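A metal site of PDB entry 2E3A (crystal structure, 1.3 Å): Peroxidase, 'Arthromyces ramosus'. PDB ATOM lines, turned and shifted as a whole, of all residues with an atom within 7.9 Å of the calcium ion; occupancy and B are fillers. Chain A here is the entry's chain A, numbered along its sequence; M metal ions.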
ATOM      1  N   PRO A 130      -3.898  -9.265 -21.269  1.00  0.00           N
ATOM      2  CA  PRO A 130      -4.204  -9.143 -19.853  1.00  0.00           C
ATOM      3  C   PRO A 130      -3.722 -10.270 -18.971  1.00  0.00           C
ATOM      4  O   PRO A 130      -3.828 -11.429 -19.298  1.00  0.00           O
ATOM      5  CB  PRO A 130      -5.728  -9.141 -19.888  1.00  0.00           C
ATOM      6  CG  PRO A 130      -6.065  -8.459 -21.167  1.00  0.00           C
ATOM      7  CD  PRO A 130      -5.042  -8.970 -22.141  1.00  0.00           C
ATOM      8  N   ALA A 182       2.469 -22.503 -20.321  1.00  0.00           N
ATOM      9  CA  ALA A 182       1.496 -21.458 -20.000  1.00  0.00           C
ATOM     10  C   ALA A 182       1.149 -20.659 -21.236  1.00  0.00           C
ATOM     11  O   ALA A 182       0.053 -20.102 -21.271  1.00  0.00           O
ATOM     12  CB  ALA A 182       2.009 -20.550 -18.897  1.00  0.00           C
ATOM     13  N   ALA A 183       1.992 -20.590 -22.270  1.00  0.00           N
ATOM     14  CA  ALA A 183       1.652 -19.930 -23.502  1.00  0.00           C
ATOM     15  C   ALA A 183       0.402 -20.513 -24.150  1.00  0.00           C
ATOM     16  O   ALA A 183      -0.289 -19.807 -24.884  1.00  0.00           O
ATOM     17  CB  ALA A 183       2.820 -20.010 -24.485  1.00  0.00           C
ATOM     18  N   HIS A 184       0.061 -21.751 -23.890  1.00  0.00           N
ATOM     19  CA  HIS A 184      -1.177 -22.339 -24.439  1.00  0.00           C
ATOM     20  C   HIS A 184      -2.400 -21.717 -23.773  1.00  0.00           C
ATOM     21  O   HIS A 184      -3.520 -22.029 -24.213  1.00  0.00           O
ATOM     22  CB  HIS A 184      -1.156 -23.860 -24.397  1.00  0.00           C
ATOM     23  CG  HIS A 184      -0.334 -24.466 -25.513  1.00  0.00           C
ATOM     24  ND1 HIS A 184      -0.392 -25.797 -25.846  1.00  0.00           N
ATOM     25  CD2 HIS A 184       0.595 -23.954 -26.350  1.00  0.00           C
ATOM     26  CE1 HIS A 184       0.455 -26.019 -26.859  1.00  0.00           C
ATOM     27  NE2 HIS A 184       1.081 -24.905 -27.203  1.00  0.00           N
ATOM     28  N   SER A 185      -2.232 -20.857 -22.768  1.00  0.00           N
ATOM     29  CA  SER A 185      -3.302 -19.997 -22.276  1.00  0.00           C
ATOM     30  C   SER A 185      -3.672 -18.886 -23.256  1.00  0.00           C
ATOM     31  O   SER A 185      -4.709 -18.252 -23.049  1.00  0.00           O
ATOM     32  CB  SER A 185      -2.904 -19.363 -20.937  1.00  0.00           C
ATOM     33  OG  SER A 185      -4.026 -18.779 -20.288  1.00  0.00           O
ATOM     34  N   LEU A 186      -2.858 -18.684 -24.293  1.00  0.00           N
ATOM     35  CA  LEU A 186      -3.125 -17.635 -25.292  1.00  0.00           C
ATOM     36  C   LEU A 186      -3.056 -18.309 -26.648  1.00  0.00           C
ATOM     37  O   LEU A 186      -2.191 -18.002 -27.448  1.00  0.00           O
ATOM     38  CB  LEU A 186      -2.081 -16.539 -25.230  1.00  0.00           C
ATOM     39  CG  LEU A 186      -2.023 -15.699 -23.956  1.00  0.00           C
ATOM     40  CD1 LEU A 186      -0.767 -14.826 -23.933  1.00  0.00           C
ATOM     41  CD2 LEU A 186      -3.256 -14.853 -23.742  1.00  0.00           C
ATOM     42  N   ALA A 187      -3.991 -19.231 -26.897  1.00  0.00           N
ATOM     43  CA  ALA A 187      -3.726 -20.151 -27.988  1.00  0.00           C
ATOM     44  C   ALA A 187      -4.954 -20.732 -28.666  1.00  0.00           C
ATOM     45  O   ALA A 187      -6.028 -20.888 -28.090  1.00  0.00           O
ATOM     46  CB  ALA A 187      -2.882 -21.310 -27.464  1.00  0.00           C
ATOM     47  N   LEU A 201      -7.455 -23.245 -27.248  1.00  0.00           N
ATOM     48  CA  LEU A 201      -6.981 -24.280 -26.323  1.00  0.00           C
ATOM     49  C   LEU A 201      -7.483 -24.039 -24.909  1.00  0.00           C
ATOM     50  O   LEU A 201      -7.485 -24.971 -24.091  1.00  0.00           O
ATOM     51  CB  LEU A 201      -5.487 -24.426 -26.342  1.00  0.00           C
ATOM     52  CG  LEU A 201      -4.785 -24.573 -27.697  1.00  0.00           C
ATOM     53  CD1 LEU A 201      -3.294 -24.780 -27.511  1.00  0.00           C
ATOM     54  CD2 LEU A 201      -5.456 -25.689 -28.495  1.00  0.00           C
ATOM     55  N   ASP A 202      -7.939 -22.830 -24.593  1.00  0.00           N
ATOM     56  CA  ASP A 202      -8.564 -22.591 -23.305  1.00  0.00           C
ATOM     57  C   ASP A 202      -9.693 -21.574 -23.553  1.00  0.00           C
ATOM     58  O   ASP A 202      -9.802 -20.955 -24.617  1.00  0.00           O
ATOM     59  CB  ASP A 202      -7.633 -22.205 -22.177  1.00  0.00           C
ATOM     60  CG  ASP A 202      -7.201 -20.774 -21.962  1.00  0.00           C
ATOM     61  OD1 ASP A 202      -7.579 -19.871 -22.744  1.00  0.00           O
ATOM     62  OD2 ASP A 202      -6.409 -20.509 -21.009  1.00  0.00           O
ATOM     63  N   SER A 203     -10.589 -21.366 -22.606  1.00  0.00           N
ATOM     64  CA  SER A 203     -11.753 -20.550 -22.727  1.00  0.00           C
ATOM     65  C   SER A 203     -11.421 -19.055 -22.772  1.00  0.00           C
ATOM     66  O   SER A 203     -12.296 -18.245 -23.084  1.00  0.00           O
ATOM     67  CB  SER A 203     -12.757 -20.794 -21.589  1.00  0.00           C
ATOM     68  OG  SER A 203     -12.250 -20.471 -20.324  1.00  0.00           O
ATOM     69  N   THR A 204     -10.172 -18.682 -22.513  1.00  0.00           N
ATOM     70  CA  THR A 204      -9.752 -17.293 -22.505  1.00  0.00           C
ATOM     71  C   THR A 204      -8.491 -17.071 -23.318  1.00  0.00           C
ATOM     72  O   THR A 204      -7.429 -16.743 -22.796  1.00  0.00           O
ATOM     73  CB  THR A 204      -9.555 -16.825 -21.054  1.00  0.00           C
ATOM     74  OG1 THR A 204      -8.576 -17.707 -20.434  1.00  0.00           O
ATOM     75  CG2 THR A 204     -10.836 -16.909 -20.248  1.00  0.00           C
ATOM     76  N   PRO A 205      -8.552 -17.230 -24.629  1.00  0.00           N
ATOM     77  CA  PRO A 205      -7.336 -17.102 -25.415  1.00  0.00           C
ATOM     78  C   PRO A 205      -6.781 -15.690 -25.516  1.00  0.00           C
ATOM     79  O   PRO A 205      -5.696 -15.578 -26.096  1.00  0.00           O
ATOM     80  CB  PRO A 205      -7.772 -17.627 -26.830  1.00  0.00           C
ATOM     81  CG  PRO A 205      -9.227 -17.293 -26.867  1.00  0.00           C
ATOM     82  CD  PRO A 205      -9.719 -17.571 -25.462  1.00  0.00           C
ATOM     83  N   GLN A 206      -7.469 -14.709 -24.943  1.00  0.00           N
ATOM     84  CA  GLN A 206      -6.924 -13.375 -24.871  1.00  0.00           C
ATOM     85  C   GLN A 206      -6.637 -12.987 -23.437  1.00  0.00           C
ATOM     86  O   GLN A 206      -6.459 -11.786 -23.144  1.00  0.00           O
ATOM     87  CB  GLN A 206      -7.912 -12.375 -25.448  1.00  0.00           C
ATOM     88  CG  GLN A 206      -8.166 -12.605 -26.934  1.00  0.00           C
ATOM     89  CD  GLN A 206      -9.033 -11.464 -27.476  1.00  0.00           C
ATOM     90  OE1 GLN A 206     -10.255 -11.487 -27.307  1.00  0.00           O
ATOM     91  NE2 GLN A 206      -8.329 -10.556 -28.117  1.00  0.00           N
ATOM     92  N   VAL A 207      -6.564 -13.932 -22.506  1.00  0.00           N
ATOM     93  CA  VAL A 207      -6.167 -13.658 -21.138  1.00  0.00           C
ATOM     94  C   VAL A 207      -5.127 -14.693 -20.704  1.00  0.00           C
ATOM     95  O   VAL A 207      -5.326 -15.902 -20.818  1.00  0.00           O
ATOM     96  CB  VAL A 207      -7.351 -13.621 -20.136  1.00  0.00           C
ATOM     97  CG1 VAL A 207      -6.845 -13.247 -18.732  1.00  0.00           C
ATOM     98  CG2 VAL A 207      -8.444 -12.672 -20.574  1.00  0.00           C
ATOM     99  N   PHE A 208      -3.997 -14.176 -20.231  1.00  0.00           N
ATOM    100  CA  PHE A 208      -2.894 -14.998 -19.774  1.00  0.00           C
ATOM    101  C   PHE A 208      -3.210 -15.421 -18.337  1.00  0.00           C
ATOM    102  O   PHE A 208      -2.922 -14.663 -17.414  1.00  0.00           O
ATOM    103  CB  PHE A 208      -1.546 -14.281 -19.853  1.00  0.00           C
ATOM    104  CG  PHE A 208      -0.408 -15.234 -19.535  1.00  0.00           C
ATOM    105  CD1 PHE A 208       0.035 -16.200 -20.417  1.00  0.00           C
ATOM    106  CD2 PHE A 208       0.248 -15.141 -18.318  1.00  0.00           C
ATOM    107  CE1 PHE A 208       1.072 -17.044 -20.072  1.00  0.00           C
ATOM    108  CE2 PHE A 208       1.289 -15.982 -17.960  1.00  0.00           C
ATOM    109  CZ  PHE A 208       1.723 -16.931 -18.868  1.00  0.00           C
ATOM    110  N   ASP A 209      -3.811 -16.575 -18.173  1.00  0.00           N
ATOM    111  CA  ASP A 209      -4.408 -17.053 -16.944  1.00  0.00           C
ATOM    112  C   ASP A 209      -4.234 -18.571 -16.841  1.00  0.00           C
ATOM    113  O   ASP A 209      -3.685 -19.247 -17.722  1.00  0.00           O
ATOM    114  CB  ASP A 209      -5.873 -16.629 -16.813  1.00  0.00           C
ATOM    115  CG  ASP A 209      -6.736 -17.141 -17.953  1.00  0.00           C
ATOM    116  OD1 ASP A 209      -6.243 -18.000 -18.706  1.00  0.00           O
ATOM    117  OD2 ASP A 209      -7.891 -16.668 -18.083  1.00  0.00           O
ATOM    118  N   THR A 210      -4.721 -19.129 -15.742  1.00  0.00           N
ATOM    119  CA  THR A 210      -4.562 -20.560 -15.484  1.00  0.00           C
ATOM    120  C   THR A 210      -5.629 -21.417 -16.162  1.00  0.00           C
ATOM    121  O   THR A 210      -5.623 -22.644 -15.923  1.00  0.00           O
ATOM    122  CB  THR A 210      -4.590 -20.839 -13.978  1.00  0.00           C
ATOM    123  OG1 THR A 210      -5.893 -20.522 -13.507  1.00  0.00           O
ATOM    124  CG2 THR A 210      -3.573 -20.020 -13.212  1.00  0.00           C
ATOM    125  N   GLN A 211      -6.548 -20.875 -16.970  1.00  0.00           N
ATOM    126  CA  GLN A 211      -7.649 -21.651 -17.493  1.00  0.00           C
ATOM    127  C   GLN A 211      -7.115 -22.842 -18.277  1.00  0.00           C
ATOM    128  O   GLN A 211      -7.690 -23.940 -18.199  1.00  0.00           O
ATOM    129  CB  GLN A 211      -8.580 -20.794 -18.358  1.00  0.00           C
ATOM    130  CG  GLN A 211      -9.437 -19.807 -17.606  1.00  0.00           C
ATOM    131  CD  GLN A 211     -10.173 -20.399 -16.439  1.00  0.00           C
ATOM    132  OE1 GLN A 211     -10.106 -19.880 -15.328  1.00  0.00           O
ATOM    133  NE2 GLN A 211     -10.903 -21.505 -16.644  1.00  0.00           N
ATOM    134  N   PHE A 212      -6.037 -22.682 -19.047  1.00  0.00           N
ATOM    135  CA  PHE A 212      -5.490 -23.795 -19.814  1.00  0.00           C
ATOM    136  C   PHE A 212      -5.201 -25.016 -18.952  1.00  0.00           C
ATOM    137  O   PHE A 212      -5.516 -26.158 -19.354  1.00  0.00           O
ATOM    138  CB  PHE A 212      -4.214 -23.312 -20.513  1.00  0.00           C
ATOM    139  CG  PHE A 212      -3.415 -24.445 -21.117  1.00  0.00           C
ATOM    140  CD1 PHE A 212      -3.855 -25.131 -22.242  1.00  0.00           C
ATOM    141  CD2 PHE A 212      -2.227 -24.810 -20.552  1.00  0.00           C
ATOM    142  CE1 PHE A 212      -3.099 -26.157 -22.781  1.00  0.00           C
ATOM    143  CE2 PHE A 212      -1.475 -25.836 -21.075  1.00  0.00           C
ATOM    144  CZ  PHE A 212      -1.921 -26.515 -22.178  1.00  0.00           C
ATOM    145  N   TYR A 213      -4.599 -24.803 -17.780  1.00  0.00           N
ATOM    146  CA  TYR A 213      -4.229 -25.925 -16.942  1.00  0.00           C
ATOM    147  C   TYR A 213      -5.458 -26.583 -16.332  1.00  0.00           C
ATOM    148  O   TYR A 213      -5.480 -27.801 -16.219  1.00  0.00           O
ATOM    149  CB  TYR A 213      -3.287 -25.419 -15.855  1.00  0.00           C
ATOM    150  CG  TYR A 213      -1.934 -24.992 -16.383  1.00  0.00           C
ATOM    151  CD1 TYR A 213      -0.966 -25.897 -16.777  1.00  0.00           C
ATOM    152  CD2 TYR A 213      -1.655 -23.638 -16.476  1.00  0.00           C
ATOM    153  CE1 TYR A 213       0.236 -25.435 -17.263  1.00  0.00           C
ATOM    154  CE2 TYR A 213      -0.442 -23.184 -16.948  1.00  0.00           C
ATOM    155  CZ  TYR A 213       0.510 -24.099 -17.334  1.00  0.00           C
ATOM    156  OH  TYR A 213       1.726 -23.633 -17.788  1.00  0.00           O
ATOM    157  N   GLU A 215      -8.589 -26.531 -17.694  1.00  0.00           N
ATOM    158  CA  GLU A 215      -9.520 -27.108 -18.662  1.00  0.00           C
ATOM    159  C   GLU A 215      -8.960 -28.340 -19.363  1.00  0.00           C
ATOM    160  O   GLU A 215      -9.736 -29.209 -19.738  1.00  0.00           O
ATOM    161  CB  GLU A 215      -9.888 -26.004 -19.648  1.00  0.00           C
ATOM    162  CG  GLU A 215     -10.780 -24.960 -19.004  1.00  0.00           C
ATOM    163  CD  GLU A 215     -10.993 -23.707 -19.799  1.00  0.00           C
ATOM    164  OE1 GLU A 215     -10.816 -23.705 -21.046  1.00  0.00           O
ATOM    165  OE2 GLU A 215     -11.345 -22.677 -19.148  1.00  0.00           O
ATOM    166  N   ASN A 266      -2.673 -17.307 -10.829  1.00  0.00           N
ATOM    167  CA  ASN A 266      -2.138 -16.597 -11.982  1.00  0.00           C
ATOM    168  C   ASN A 266      -0.751 -16.016 -11.651  1.00  0.00           C
ATOM    169  O   ASN A 266       0.092 -15.918 -12.518  1.00  0.00           O
ATOM    170  CB  ASN A 266      -3.099 -15.492 -12.400  1.00  0.00           C
ATOM    171  CG  ASN A 266      -4.382 -16.000 -13.024  1.00  0.00           C
ATOM    172  OD1 ASN A 266      -4.402 -16.932 -13.810  1.00  0.00           O
ATOM    173  ND2 ASN A 266      -5.497 -15.390 -12.670  1.00  0.00           N
ATOM    174  N   MET A 269       1.932 -18.733 -11.705  1.00  0.00           N
ATOM    175  CA  MET A 269       2.094 -19.139 -13.088  1.00  0.00           C
ATOM    176  C   MET A 269       2.910 -18.124 -13.858  1.00  0.00           C
ATOM    177  O   MET A 269       3.833 -18.493 -14.608  1.00  0.00           O
ATOM    178  CB  MET A 269       0.731 -19.315 -13.762  1.00  0.00           C
ATOM    179  CG  MET A 269       0.831 -19.646 -15.236  1.00  0.00           C
ATOM    180  SD  MET A 269      -0.777 -19.630 -16.082  1.00  0.00           S
ATOM    181  CE  MET A 269      -1.023 -17.860 -16.159  1.00  0.00           C
ATOM    182  N   ASN A 303      -5.195  -8.626 -14.969  1.00  0.00           N
ATOM    183  CA  ASN A 303      -6.352  -9.499 -15.099  1.00  0.00           C
ATOM    184  C   ASN A 303      -7.017  -9.640 -13.732  1.00  0.00           C
ATOM    185  O   ASN A 303      -6.358 -10.131 -12.802  1.00  0.00           O
ATOM    186  CB  ASN A 303      -5.968 -10.897 -15.611  1.00  0.00           C
ATOM    187  CG  ASN A 303      -7.129 -11.864 -15.525  1.00  0.00           C
ATOM    188  OD1 ASN A 303      -8.295 -11.497 -15.704  1.00  0.00           O
ATOM    189  ND2 ASN A 303      -6.846 -13.124 -15.219  1.00  0.00           N
HETATM  190 CA    CA M   1      -6.226 -18.104 -21.197  1.00  0.00          CA
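The side-chain carboxylate of Asp 209 sits close to the backbone NH of Gln 211, 3.4 Å away. The side-chain carboxylate (OD2) of Asp 202 lies close to the backbone NH (N) of Phe 212, at 3.0 Å.
The calcium ion is bound by the backbone carbonyl oxygen (O) of Ser 185, at 2.4 Å. O of Val 207 is bound to the calcium ion. The calcium ion is bound by OD2 of Asp 202, 2.4 Å away. O of Thr 204 is bound to the calcium ion, 2.4 Å away. OG of Ser 185 is bound to the calcium ion. OD1 of Asp 209 binds the calcium ion (2.5 Å). The calcium ion is bound by OG1 of Thr 204. The calcium ion is bound by the side-chain carboxylate (OD1) of Asp 202, at 2.7 Å. The calcium ion has eight donor atoms within binding distance.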
